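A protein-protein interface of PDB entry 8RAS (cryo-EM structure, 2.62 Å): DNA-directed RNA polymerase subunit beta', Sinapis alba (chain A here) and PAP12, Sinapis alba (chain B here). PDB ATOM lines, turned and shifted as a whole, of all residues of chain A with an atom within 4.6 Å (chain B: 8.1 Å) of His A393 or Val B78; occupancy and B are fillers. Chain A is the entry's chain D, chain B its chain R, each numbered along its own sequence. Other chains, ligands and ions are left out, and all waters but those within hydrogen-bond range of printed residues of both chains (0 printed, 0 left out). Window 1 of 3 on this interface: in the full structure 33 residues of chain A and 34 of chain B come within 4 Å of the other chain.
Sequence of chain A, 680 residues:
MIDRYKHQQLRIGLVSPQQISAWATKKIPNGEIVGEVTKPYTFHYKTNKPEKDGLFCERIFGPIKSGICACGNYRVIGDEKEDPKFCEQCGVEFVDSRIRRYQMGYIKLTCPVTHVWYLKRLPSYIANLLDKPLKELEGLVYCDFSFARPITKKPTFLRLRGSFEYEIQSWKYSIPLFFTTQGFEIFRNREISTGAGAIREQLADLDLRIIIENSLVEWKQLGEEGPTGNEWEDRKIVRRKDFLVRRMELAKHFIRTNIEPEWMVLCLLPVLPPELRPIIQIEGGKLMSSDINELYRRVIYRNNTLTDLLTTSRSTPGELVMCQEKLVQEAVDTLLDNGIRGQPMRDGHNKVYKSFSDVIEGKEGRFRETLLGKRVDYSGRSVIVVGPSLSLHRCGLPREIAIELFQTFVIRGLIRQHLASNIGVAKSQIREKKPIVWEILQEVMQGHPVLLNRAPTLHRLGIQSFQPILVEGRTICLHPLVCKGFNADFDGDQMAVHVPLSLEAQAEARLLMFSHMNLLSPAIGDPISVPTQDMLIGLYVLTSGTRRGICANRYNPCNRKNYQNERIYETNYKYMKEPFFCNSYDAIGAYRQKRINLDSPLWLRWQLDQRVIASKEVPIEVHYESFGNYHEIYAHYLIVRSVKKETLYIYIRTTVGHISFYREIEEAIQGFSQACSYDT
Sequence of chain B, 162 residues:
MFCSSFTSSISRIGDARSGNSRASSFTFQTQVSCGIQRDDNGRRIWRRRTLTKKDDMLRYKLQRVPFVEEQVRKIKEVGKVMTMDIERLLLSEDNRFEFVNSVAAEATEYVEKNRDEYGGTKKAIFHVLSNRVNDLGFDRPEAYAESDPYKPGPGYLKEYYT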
ATOM      1  N   SER A 391      -5.034 -32.074 -17.910  1.00  0.00           N
ATOM      2  CA  SER A 391      -5.077 -31.985 -19.357  1.00  0.00           C
ATOM      3  C   SER A 391      -3.925 -31.118 -19.856  1.00  0.00           C
ATOM      4  O   SER A 391      -3.282 -30.391 -19.094  1.00  0.00           O
ATOM      5  CB  SER A 391      -6.416 -31.421 -19.822  1.00  0.00           C
ATOM      6  OG  SER A 391      -7.494 -32.112 -19.218  1.00  0.00           O
ATOM      7  N   LEU A 392      -3.659 -31.206 -21.160  1.00  0.00           N
ATOM      8  CA  LEU A 392      -2.562 -30.441 -21.739  1.00  0.00           C
ATOM      9  C   LEU A 392      -2.802 -28.939 -21.671  1.00  0.00           C
ATOM     10  O   LEU A 392      -1.840 -28.167 -21.734  1.00  0.00           O
ATOM     11  CB  LEU A 392      -2.333 -30.870 -23.188  1.00  0.00           C
ATOM     12  CG  LEU A 392      -0.970 -30.548 -23.802  1.00  0.00           C
ATOM     13  CD1 LEU A 392       0.134 -30.666 -22.765  1.00  0.00           C
ATOM     14  CD2 LEU A 392      -0.697 -31.463 -24.979  1.00  0.00           C
ATOM     15  N   HIS A 393      -4.054 -28.508 -21.531  1.00  0.00           N
ATOM     16  CA  HIS A 393      -4.402 -27.094 -21.517  1.00  0.00           C
ATOM     17  C   HIS A 393      -4.805 -26.593 -20.136  1.00  0.00           C
ATOM     18  O   HIS A 393      -5.374 -25.503 -20.029  1.00  0.00           O
ATOM     19  CB  HIS A 393      -5.531 -26.825 -22.513  1.00  0.00           C
ATOM     20  CG  HIS A 393      -6.846 -27.412 -22.107  1.00  0.00           C
ATOM     21  ND1 HIS A 393      -7.182 -28.725 -22.355  1.00  0.00           N
ATOM     22  CD2 HIS A 393      -7.908 -26.868 -21.466  1.00  0.00           C
ATOM     23  CE1 HIS A 393      -8.394 -28.964 -21.886  1.00  0.00           C
ATOM     24  NE2 HIS A 393      -8.856 -27.853 -21.343  1.00  0.00           N
ATOM     25  N   ARG A 394      -4.524 -27.350 -19.080  1.00  0.00           N
ATOM     26  CA  ARG A 394      -4.956 -26.993 -17.738  1.00  0.00           C
ATOM     27  C   ARG A 394      -3.770 -26.926 -16.786  1.00  0.00           C
ATOM     28  O   ARG A 394      -2.737 -27.563 -17.003  1.00  0.00           O
ATOM     29  CB  ARG A 394      -5.983 -27.992 -17.199  1.00  0.00           C
ATOM     30  CG  ARG A 394      -7.413 -27.669 -17.572  1.00  0.00           C
ATOM     31  CD  ARG A 394      -8.299 -28.885 -17.420  1.00  0.00           C
ATOM     32  NE  ARG A 394      -9.689 -28.519 -17.178  1.00  0.00           N
ATOM     33  CZ  ARG A 394     -10.524 -29.218 -16.423  1.00  0.00           C
ATOM     34  NH1 ARG A 394     -10.139 -30.325 -15.810  1.00  0.00           N
ATOM     35  NH2 ARG A 394     -11.775 -28.794 -16.276  1.00  0.00           N
ATOM     36  N   CYS A 395      -3.936 -26.136 -15.729  1.00  0.00           N
ATOM     37  CA  CYS A 395      -2.966 -26.045 -14.651  1.00  0.00           C
ATOM     38  C   CYS A 395      -3.714 -25.956 -13.330  1.00  0.00           C
ATOM     39  O   CYS A 395      -4.891 -25.594 -13.284  1.00  0.00           O
ATOM     40  CB  CYS A 395      -2.031 -24.839 -14.823  1.00  0.00           C
ATOM     41  SG  CYS A 395      -2.754 -23.251 -14.372  1.00  0.00           S
ATOM     42  N   PHE A 466      -2.666 -21.304 -19.613  1.00  0.00           N
ATOM     43  CA  PHE A 466      -3.382 -22.500 -19.201  1.00  0.00           C
ATOM     44  C   PHE A 466      -4.724 -22.102 -18.607  1.00  0.00           C
ATOM     45  O   PHE A 466      -4.957 -20.941 -18.267  1.00  0.00           O
ATOM     46  CB  PHE A 466      -2.586 -23.318 -18.174  1.00  0.00           C
ATOM     47  CG  PHE A 466      -1.251 -23.783 -18.674  1.00  0.00           C
ATOM     48  CD1 PHE A 466      -0.126 -22.990 -18.523  1.00  0.00           C
ATOM     49  CD2 PHE A 466      -1.120 -25.013 -19.291  1.00  0.00           C
ATOM     50  CE1 PHE A 466       1.100 -23.415 -18.982  1.00  0.00           C
ATOM     51  CE2 PHE A 466       0.104 -25.442 -19.751  1.00  0.00           C
ATOM     52  CZ  PHE A 466       1.216 -24.642 -19.596  1.00  0.00           C
ATOM     53  N   GLN A 467      -5.611 -23.088 -18.489  1.00  0.00           N
ATOM     54  CA  GLN A 467      -6.892 -22.887 -17.828  1.00  0.00           C
ATOM     55  C   GLN A 467      -6.742 -23.266 -16.362  1.00  0.00           C
ATOM     56  O   GLN A 467      -6.527 -24.448 -16.058  1.00  0.00           O
ATOM     57  CB  GLN A 467      -7.975 -23.726 -18.490  1.00  0.00           C
ATOM     58  CG  GLN A 467      -9.301 -23.725 -17.754  1.00  0.00           C
ATOM     59  CD  GLN A 467      -9.824 -22.329 -17.496  1.00  0.00           C
ATOM     60  OE1 GLN A 467     -10.189 -21.989 -16.372  1.00  0.00           O
ATOM     61  NE2 GLN A 467      -9.864 -21.510 -18.538  1.00  0.00           N
ATOM     62  N   PHE A 514      -2.032 -20.725 -25.705  1.00  0.00           N
ATOM     63  CA  PHE A 514      -2.343 -22.027 -25.132  1.00  0.00           C
ATOM     64  C   PHE A 514      -1.446 -23.103 -25.732  1.00  0.00           C
ATOM     65  O   PHE A 514      -1.011 -23.015 -26.883  1.00  0.00           O
ATOM     66  CB  PHE A 514      -3.813 -22.380 -25.350  1.00  0.00           C
ATOM     67  CG  PHE A 514      -4.677 -22.120 -24.155  1.00  0.00           C
ATOM     68  CD1 PHE A 514      -4.674 -20.883 -23.538  1.00  0.00           C
ATOM     69  CD2 PHE A 514      -5.490 -23.114 -23.644  1.00  0.00           C
ATOM     70  CE1 PHE A 514      -5.467 -20.641 -22.438  1.00  0.00           C
ATOM     71  CE2 PHE A 514      -6.284 -22.877 -22.544  1.00  0.00           C
ATOM     72  CZ  PHE A 514      -6.273 -21.640 -21.940  1.00  0.00           C
ATOM     73  N   GLN B  71     -14.001 -41.635 -22.754  1.00  0.00           N
ATOM     74  CA  GLN B  71     -13.088 -40.720 -23.428  1.00  0.00           C
ATOM     75  C   GLN B  71     -13.827 -39.506 -23.980  1.00  0.00           C
ATOM     76  O   GLN B  71     -13.403 -38.363 -23.773  1.00  0.00           O
ATOM     77  CB  GLN B  71     -12.361 -41.462 -24.543  1.00  0.00           C
ATOM     78  CG  GLN B  71     -10.913 -41.082 -24.700  1.00  0.00           C
ATOM     79  CD  GLN B  71     -10.329 -41.620 -25.978  1.00  0.00           C
ATOM     80  OE1 GLN B  71     -10.583 -42.761 -26.360  1.00  0.00           O
ATOM     81  NE2 GLN B  71      -9.543 -40.802 -26.652  1.00  0.00           N
ATOM     82  N   VAL B  72     -14.936 -39.736 -24.684  1.00  0.00           N
ATOM     83  CA  VAL B  72     -15.715 -38.634 -25.242  1.00  0.00           C
ATOM     84  C   VAL B  72     -16.271 -37.756 -24.130  1.00  0.00           C
ATOM     85  O   VAL B  72     -16.238 -36.520 -24.214  1.00  0.00           O
ATOM     86  CB  VAL B  72     -16.836 -39.182 -26.147  1.00  0.00           C
ATOM     87  CG1 VAL B  72     -17.845 -38.093 -26.466  1.00  0.00           C
ATOM     88  CG2 VAL B  72     -16.252 -39.763 -27.422  1.00  0.00           C
ATOM     89  N   ARG B  73     -16.794 -38.379 -23.071  1.00  0.00           N
ATOM     90  CA  ARG B  73     -17.339 -37.607 -21.963  1.00  0.00           C
ATOM     91  C   ARG B  73     -16.262 -36.763 -21.293  1.00  0.00           C
ATOM     92  O   ARG B  73     -16.498 -35.600 -20.955  1.00  0.00           O
ATOM     93  CB  ARG B  73     -18.000 -38.539 -20.952  1.00  0.00           C
ATOM     94  CG  ARG B  73     -18.656 -37.825 -19.790  1.00  0.00           C
ATOM     95  CD  ARG B  73     -19.352 -38.809 -18.875  1.00  0.00           C
ATOM     96  NE  ARG B  73     -18.510 -39.963 -18.585  1.00  0.00           N
ATOM     97  CZ  ARG B  73     -18.766 -41.197 -18.995  1.00  0.00           C
ATOM     98  NH1 ARG B  73     -19.829 -41.475 -19.732  1.00  0.00           N
ATOM     99  NH2 ARG B  73     -17.934 -42.176 -18.659  1.00  0.00           N
ATOM    100  N   LYS B  74     -15.069 -37.329 -21.102  1.00  0.00           N
ATOM    101  CA  LYS B  74     -13.979 -36.578 -20.492  1.00  0.00           C
ATOM    102  C   LYS B  74     -13.535 -35.432 -21.393  1.00  0.00           C
ATOM    103  O   LYS B  74     -13.224 -34.338 -20.906  1.00  0.00           O
ATOM    104  CB  LYS B  74     -12.813 -37.523 -20.188  1.00  0.00           C
ATOM    105  CG  LYS B  74     -11.507 -36.854 -19.779  1.00  0.00           C
ATOM    106  CD  LYS B  74     -11.680 -35.911 -18.592  1.00  0.00           C
ATOM    107  CE  LYS B  74     -12.309 -36.610 -17.394  1.00  0.00           C
ATOM    108  NZ  LYS B  74     -13.168 -35.690 -16.600  1.00  0.00           N
ATOM    109  N   ILE B  75     -13.507 -35.662 -22.709  1.00  0.00           N
ATOM    110  CA  ILE B  75     -13.162 -34.598 -23.649  1.00  0.00           C
ATOM    111  C   ILE B  75     -14.153 -33.450 -23.529  1.00  0.00           C
ATOM    112  O   ILE B  75     -13.773 -32.275 -23.485  1.00  0.00           O
ATOM    113  CB  ILE B  75     -13.113 -35.142 -25.088  1.00  0.00           C
ATOM    114  CG1 ILE B  75     -11.866 -35.996 -25.305  1.00  0.00           C
ATOM    115  CG2 ILE B  75     -13.133 -34.004 -26.091  1.00  0.00           C
ATOM    116  CD1 ILE B  75     -11.833 -36.665 -26.656  1.00  0.00           C
ATOM    117  N   LYS B  76     -15.445 -33.778 -23.468  1.00  0.00           N
ATOM    118  CA  LYS B  76     -16.457 -32.739 -23.314  1.00  0.00           C
ATOM    119  C   LYS B  76     -16.317 -32.021 -21.976  1.00  0.00           C
ATOM    120  O   LYS B  76     -16.491 -30.798 -21.899  1.00  0.00           O
ATOM    121  CB  LYS B  76     -17.854 -33.339 -23.462  1.00  0.00           C
ATOM    122  CG  LYS B  76     -18.351 -33.374 -24.896  1.00  0.00           C
ATOM    123  CD  LYS B  76     -18.911 -34.736 -25.259  1.00  0.00           C
ATOM    124  CE  LYS B  76     -19.538 -34.719 -26.642  1.00  0.00           C
ATOM    125  NZ  LYS B  76     -20.884 -34.084 -26.633  1.00  0.00           N
ATOM    126  N   GLU B  77     -16.005 -32.762 -20.910  1.00  0.00           N
ATOM    127  CA  GLU B  77     -15.875 -32.150 -19.590  1.00  0.00           C
ATOM    128  C   GLU B  77     -14.706 -31.175 -19.528  1.00  0.00           C
ATOM    129  O   GLU B  77     -14.831 -30.089 -18.951  1.00  0.00           O
ATOM    130  CB  GLU B  77     -15.722 -33.229 -18.518  1.00  0.00           C
ATOM    131  CG  GLU B  77     -16.960 -34.080 -18.299  1.00  0.00           C
ATOM    132  CD  GLU B  77     -16.702 -35.244 -17.362  1.00  0.00           C
ATOM    133  OE1 GLU B  77     -15.602 -35.300 -16.773  1.00  0.00           O
ATOM    134  OE2 GLU B  77     -17.596 -36.102 -17.216  1.00  0.00           O
ATOM    135  N   VAL B  78     -13.558 -31.540 -20.105  1.00  0.00           N
ATOM    136  CA  VAL B  78     -12.392 -30.666 -19.996  1.00  0.00           C
ATOM    137  C   VAL B  78     -12.438 -29.505 -20.981  1.00  0.00           C
ATOM    138  O   VAL B  78     -11.801 -28.474 -20.737  1.00  0.00           O
ATOM    139  CB  VAL B  78     -11.083 -31.450 -20.182  1.00  0.00           C
ATOM    140  CG1 VAL B  78     -10.921 -32.471 -19.076  1.00  0.00           C
ATOM    141  CG2 VAL B  78     -11.043 -32.118 -21.545  1.00  0.00           C
ATOM    142  N   GLY B  79     -13.172 -29.635 -22.081  1.00  0.00           N
ATOM    143  CA  GLY B  79     -13.276 -28.557 -23.041  1.00  0.00           C
ATOM    144  C   GLY B  79     -12.246 -28.610 -24.150  1.00  0.00           C
ATOM    145  O   GLY B  79     -11.595 -27.604 -24.447  1.00  0.00           O
ATOM    146  N   LYS B  80     -12.084 -29.779 -24.768  1.00  0.00           N
ATOM    147  CA  LYS B  80     -11.230 -29.912 -25.940  1.00  0.00           C
ATOM    148  C   LYS B  80     -11.989 -29.676 -27.236  1.00  0.00           C
ATOM    149  O   LYS B  80     -11.370 -29.364 -28.265  1.00  0.00           O
ATOM    150  CB  LYS B  80     -10.583 -31.299 -25.960  1.00  0.00           C
ATOM    151  CG  LYS B  80      -9.583 -31.516 -24.839  1.00  0.00           C
ATOM    152  CD  LYS B  80      -8.935 -32.886 -24.918  1.00  0.00           C
ATOM    153  CE  LYS B  80      -7.654 -32.925 -24.103  1.00  0.00           C
ATOM    154  NZ  LYS B  80      -7.046 -34.280 -24.071  1.00  0.00           N
ATOM    155  N   VAL B  81     -13.317 -29.808 -27.198  1.00  0.00           N
ATOM    156  CA  VAL B  81     -14.143 -29.444 -28.341  1.00  0.00           C
ATOM    157  C   VAL B  81     -13.953 -27.977 -28.681  1.00  0.00           C
ATOM    158  O   VAL B  81     -13.984 -27.593 -29.854  1.00  0.00           O
ATOM    159  CB  VAL B  81     -15.621 -29.774 -28.057  1.00  0.00           C
ATOM    160  CG1 VAL B  81     -16.452 -29.611 -29.311  1.00  0.00           C
ATOM    161  CG2 VAL B  81     -15.749 -31.184 -27.509  1.00  0.00           C
ATOM    162  N   MET B  82     -13.743 -27.132 -27.668  1.00  0.00           N
ATOM    163  CA  MET B  82     -13.455 -25.729 -27.938  1.00  0.00           C
ATOM    164  C   MET B  82     -12.116 -25.564 -28.644  1.00  0.00           C
ATOM    165  O   MET B  82     -11.967 -24.684 -29.495  1.00  0.00           O
ATOM    166  CB  MET B  82     -13.471 -24.918 -26.646  1.00  0.00           C
ATOM    167  CG  MET B  82     -13.231 -23.442 -26.885  1.00  0.00           C
ATOM    168  SD  MET B  82     -13.740 -22.367 -25.542  1.00  0.00           S
ATOM    169  CE  MET B  82     -12.302 -21.308 -25.461  1.00  0.00           C
ATOM    170  N   THR B  83     -11.124 -26.385 -28.296  1.00  0.00           N
ATOM    171  CA  THR B  83      -9.850 -26.335 -29.007  1.00  0.00           C
ATOM    172  C   THR B  83     -10.027 -26.719 -30.470  1.00  0.00           C
ATOM    173  O   THR B  83      -9.465 -26.074 -31.367  1.00  0.00           O
ATOM    174  CB  THR B  83      -8.831 -27.252 -28.331  1.00  0.00           C
ATOM    175  OG1 THR B  83      -9.089 -28.611 -28.702  1.00  0.00           O
ATOM    176  CG2 THR B  83      -8.923 -27.127 -26.821  1.00  0.00           C
ATOM    177  N   PHE B 126     -16.013 -16.937 -24.864  1.00  0.00           N
ATOM    178  CA  PHE B 126     -16.584 -18.252 -25.129  1.00  0.00           C
ATOM    179  C   PHE B 126     -17.885 -18.130 -25.910  1.00  0.00           C
ATOM    180  O   PHE B 126     -18.146 -18.919 -26.826  1.00  0.00           O
ATOM    181  CB  PHE B 126     -16.815 -19.001 -23.817  1.00  0.00           C
ATOM    182  CG  PHE B 126     -15.568 -19.589 -23.220  1.00  0.00           C
ATOM    183  CD1 PHE B 126     -14.363 -18.910 -23.272  1.00  0.00           C
ATOM    184  CD2 PHE B 126     -15.603 -20.827 -22.606  1.00  0.00           C
ATOM    185  CE1 PHE B 126     -13.223 -19.450 -22.723  1.00  0.00           C
ATOM    186  CE2 PHE B 126     -14.465 -21.374 -22.057  1.00  0.00           C
ATOM    187  CZ  PHE B 126     -13.273 -20.686 -22.118  1.00  0.00           C
ATOM    188  N   GLU B 146     -21.020 -25.396 -18.958  1.00  0.00           N
ATOM    189  CA  GLU B 146     -21.439 -26.688 -18.439  1.00  0.00           C
ATOM    190  C   GLU B 146     -21.225 -26.719 -16.934  1.00  0.00           C
ATOM    191  O   GLU B 146     -20.365 -26.017 -16.398  1.00  0.00           O
ATOM    192  CB  GLU B 146     -20.673 -27.842 -19.101  1.00  0.00           C
ATOM    193  CG  GLU B 146     -21.101 -28.139 -20.530  1.00  0.00           C
ATOM    194  CD  GLU B 146     -20.206 -29.163 -21.204  1.00  0.00           C
ATOM    195  OE1 GLU B 146     -19.152 -29.504 -20.627  1.00  0.00           O
ATOM    196  OE2 GLU B 146     -20.557 -29.627 -22.309  1.00  0.00           O
ATOM    197  N   TYR B 160     -10.166 -31.622  -6.700  1.00  0.00           N
ATOM    198  CA  TYR B 160      -9.433 -32.245  -7.792  1.00  0.00           C
ATOM    199  C   TYR B 160      -8.568 -33.393  -7.283  1.00  0.00           C
ATOM    200  O   TYR B 160      -7.376 -33.462  -7.574  1.00  0.00           O
ATOM    201  CB  TYR B 160      -8.569 -31.215  -8.517  1.00  0.00           C
ATOM    202  CG  TYR B 160      -8.257 -31.588  -9.946  1.00  0.00           C
ATOM    203  CD1 TYR B 160      -9.274 -31.827 -10.858  1.00  0.00           C
ATOM    204  CD2 TYR B 160      -6.944 -31.717 -10.379  1.00  0.00           C
ATOM    205  CE1 TYR B 160      -8.994 -32.174 -12.164  1.00  0.00           C
ATOM    206  CE2 TYR B 160      -6.655 -32.066 -11.683  1.00  0.00           C
ATOM    207  CZ  TYR B 160      -7.683 -32.292 -12.570  1.00  0.00           C
ATOM    208  OH  TYR B 160      -7.400 -32.638 -13.870  1.00  0.00           O
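The backbone carbonyl oxygen of Val B78 sits at hydrogen-bond distance from a ring nitrogen (NE2) of His A393 (3.1 Å).
The backbone carbonyl oxygen of His A393 lies within hydrogen-bond range of the backbone NH of Gln A467 (2.9 Å).
OG of Ser A391 touches CG1 of Val B78, at 3.4 Å.
Val B78 touches Arg A394.
Of the printed residues of chain B, Ser A391 touches Val B78.
Printed residues of chain B within 4 Å of Arg A394: Val B78 (3.99 Å).
Of the printed residues of chain A, Val B78 touches Ser A391, His A393 and Arg A394.
The nearest printed residue of chain A that does not touch Val B78 is Gln A467 (6.1 Å).
Of the 16 printed residues of chain B, 1 touches a printed residue of chain A.
Of the 8 printed residues of chain A, 3 touch a printed residue of chain B.
Printed residues of chain A that touch a printed residue of chain B: Ser A391, His A393 and Arg A394.
Among the printed residues, no Asp or Glu carboxylate lies within 4 Å of a Lys or Arg side-chain nitrogen of the other chain.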
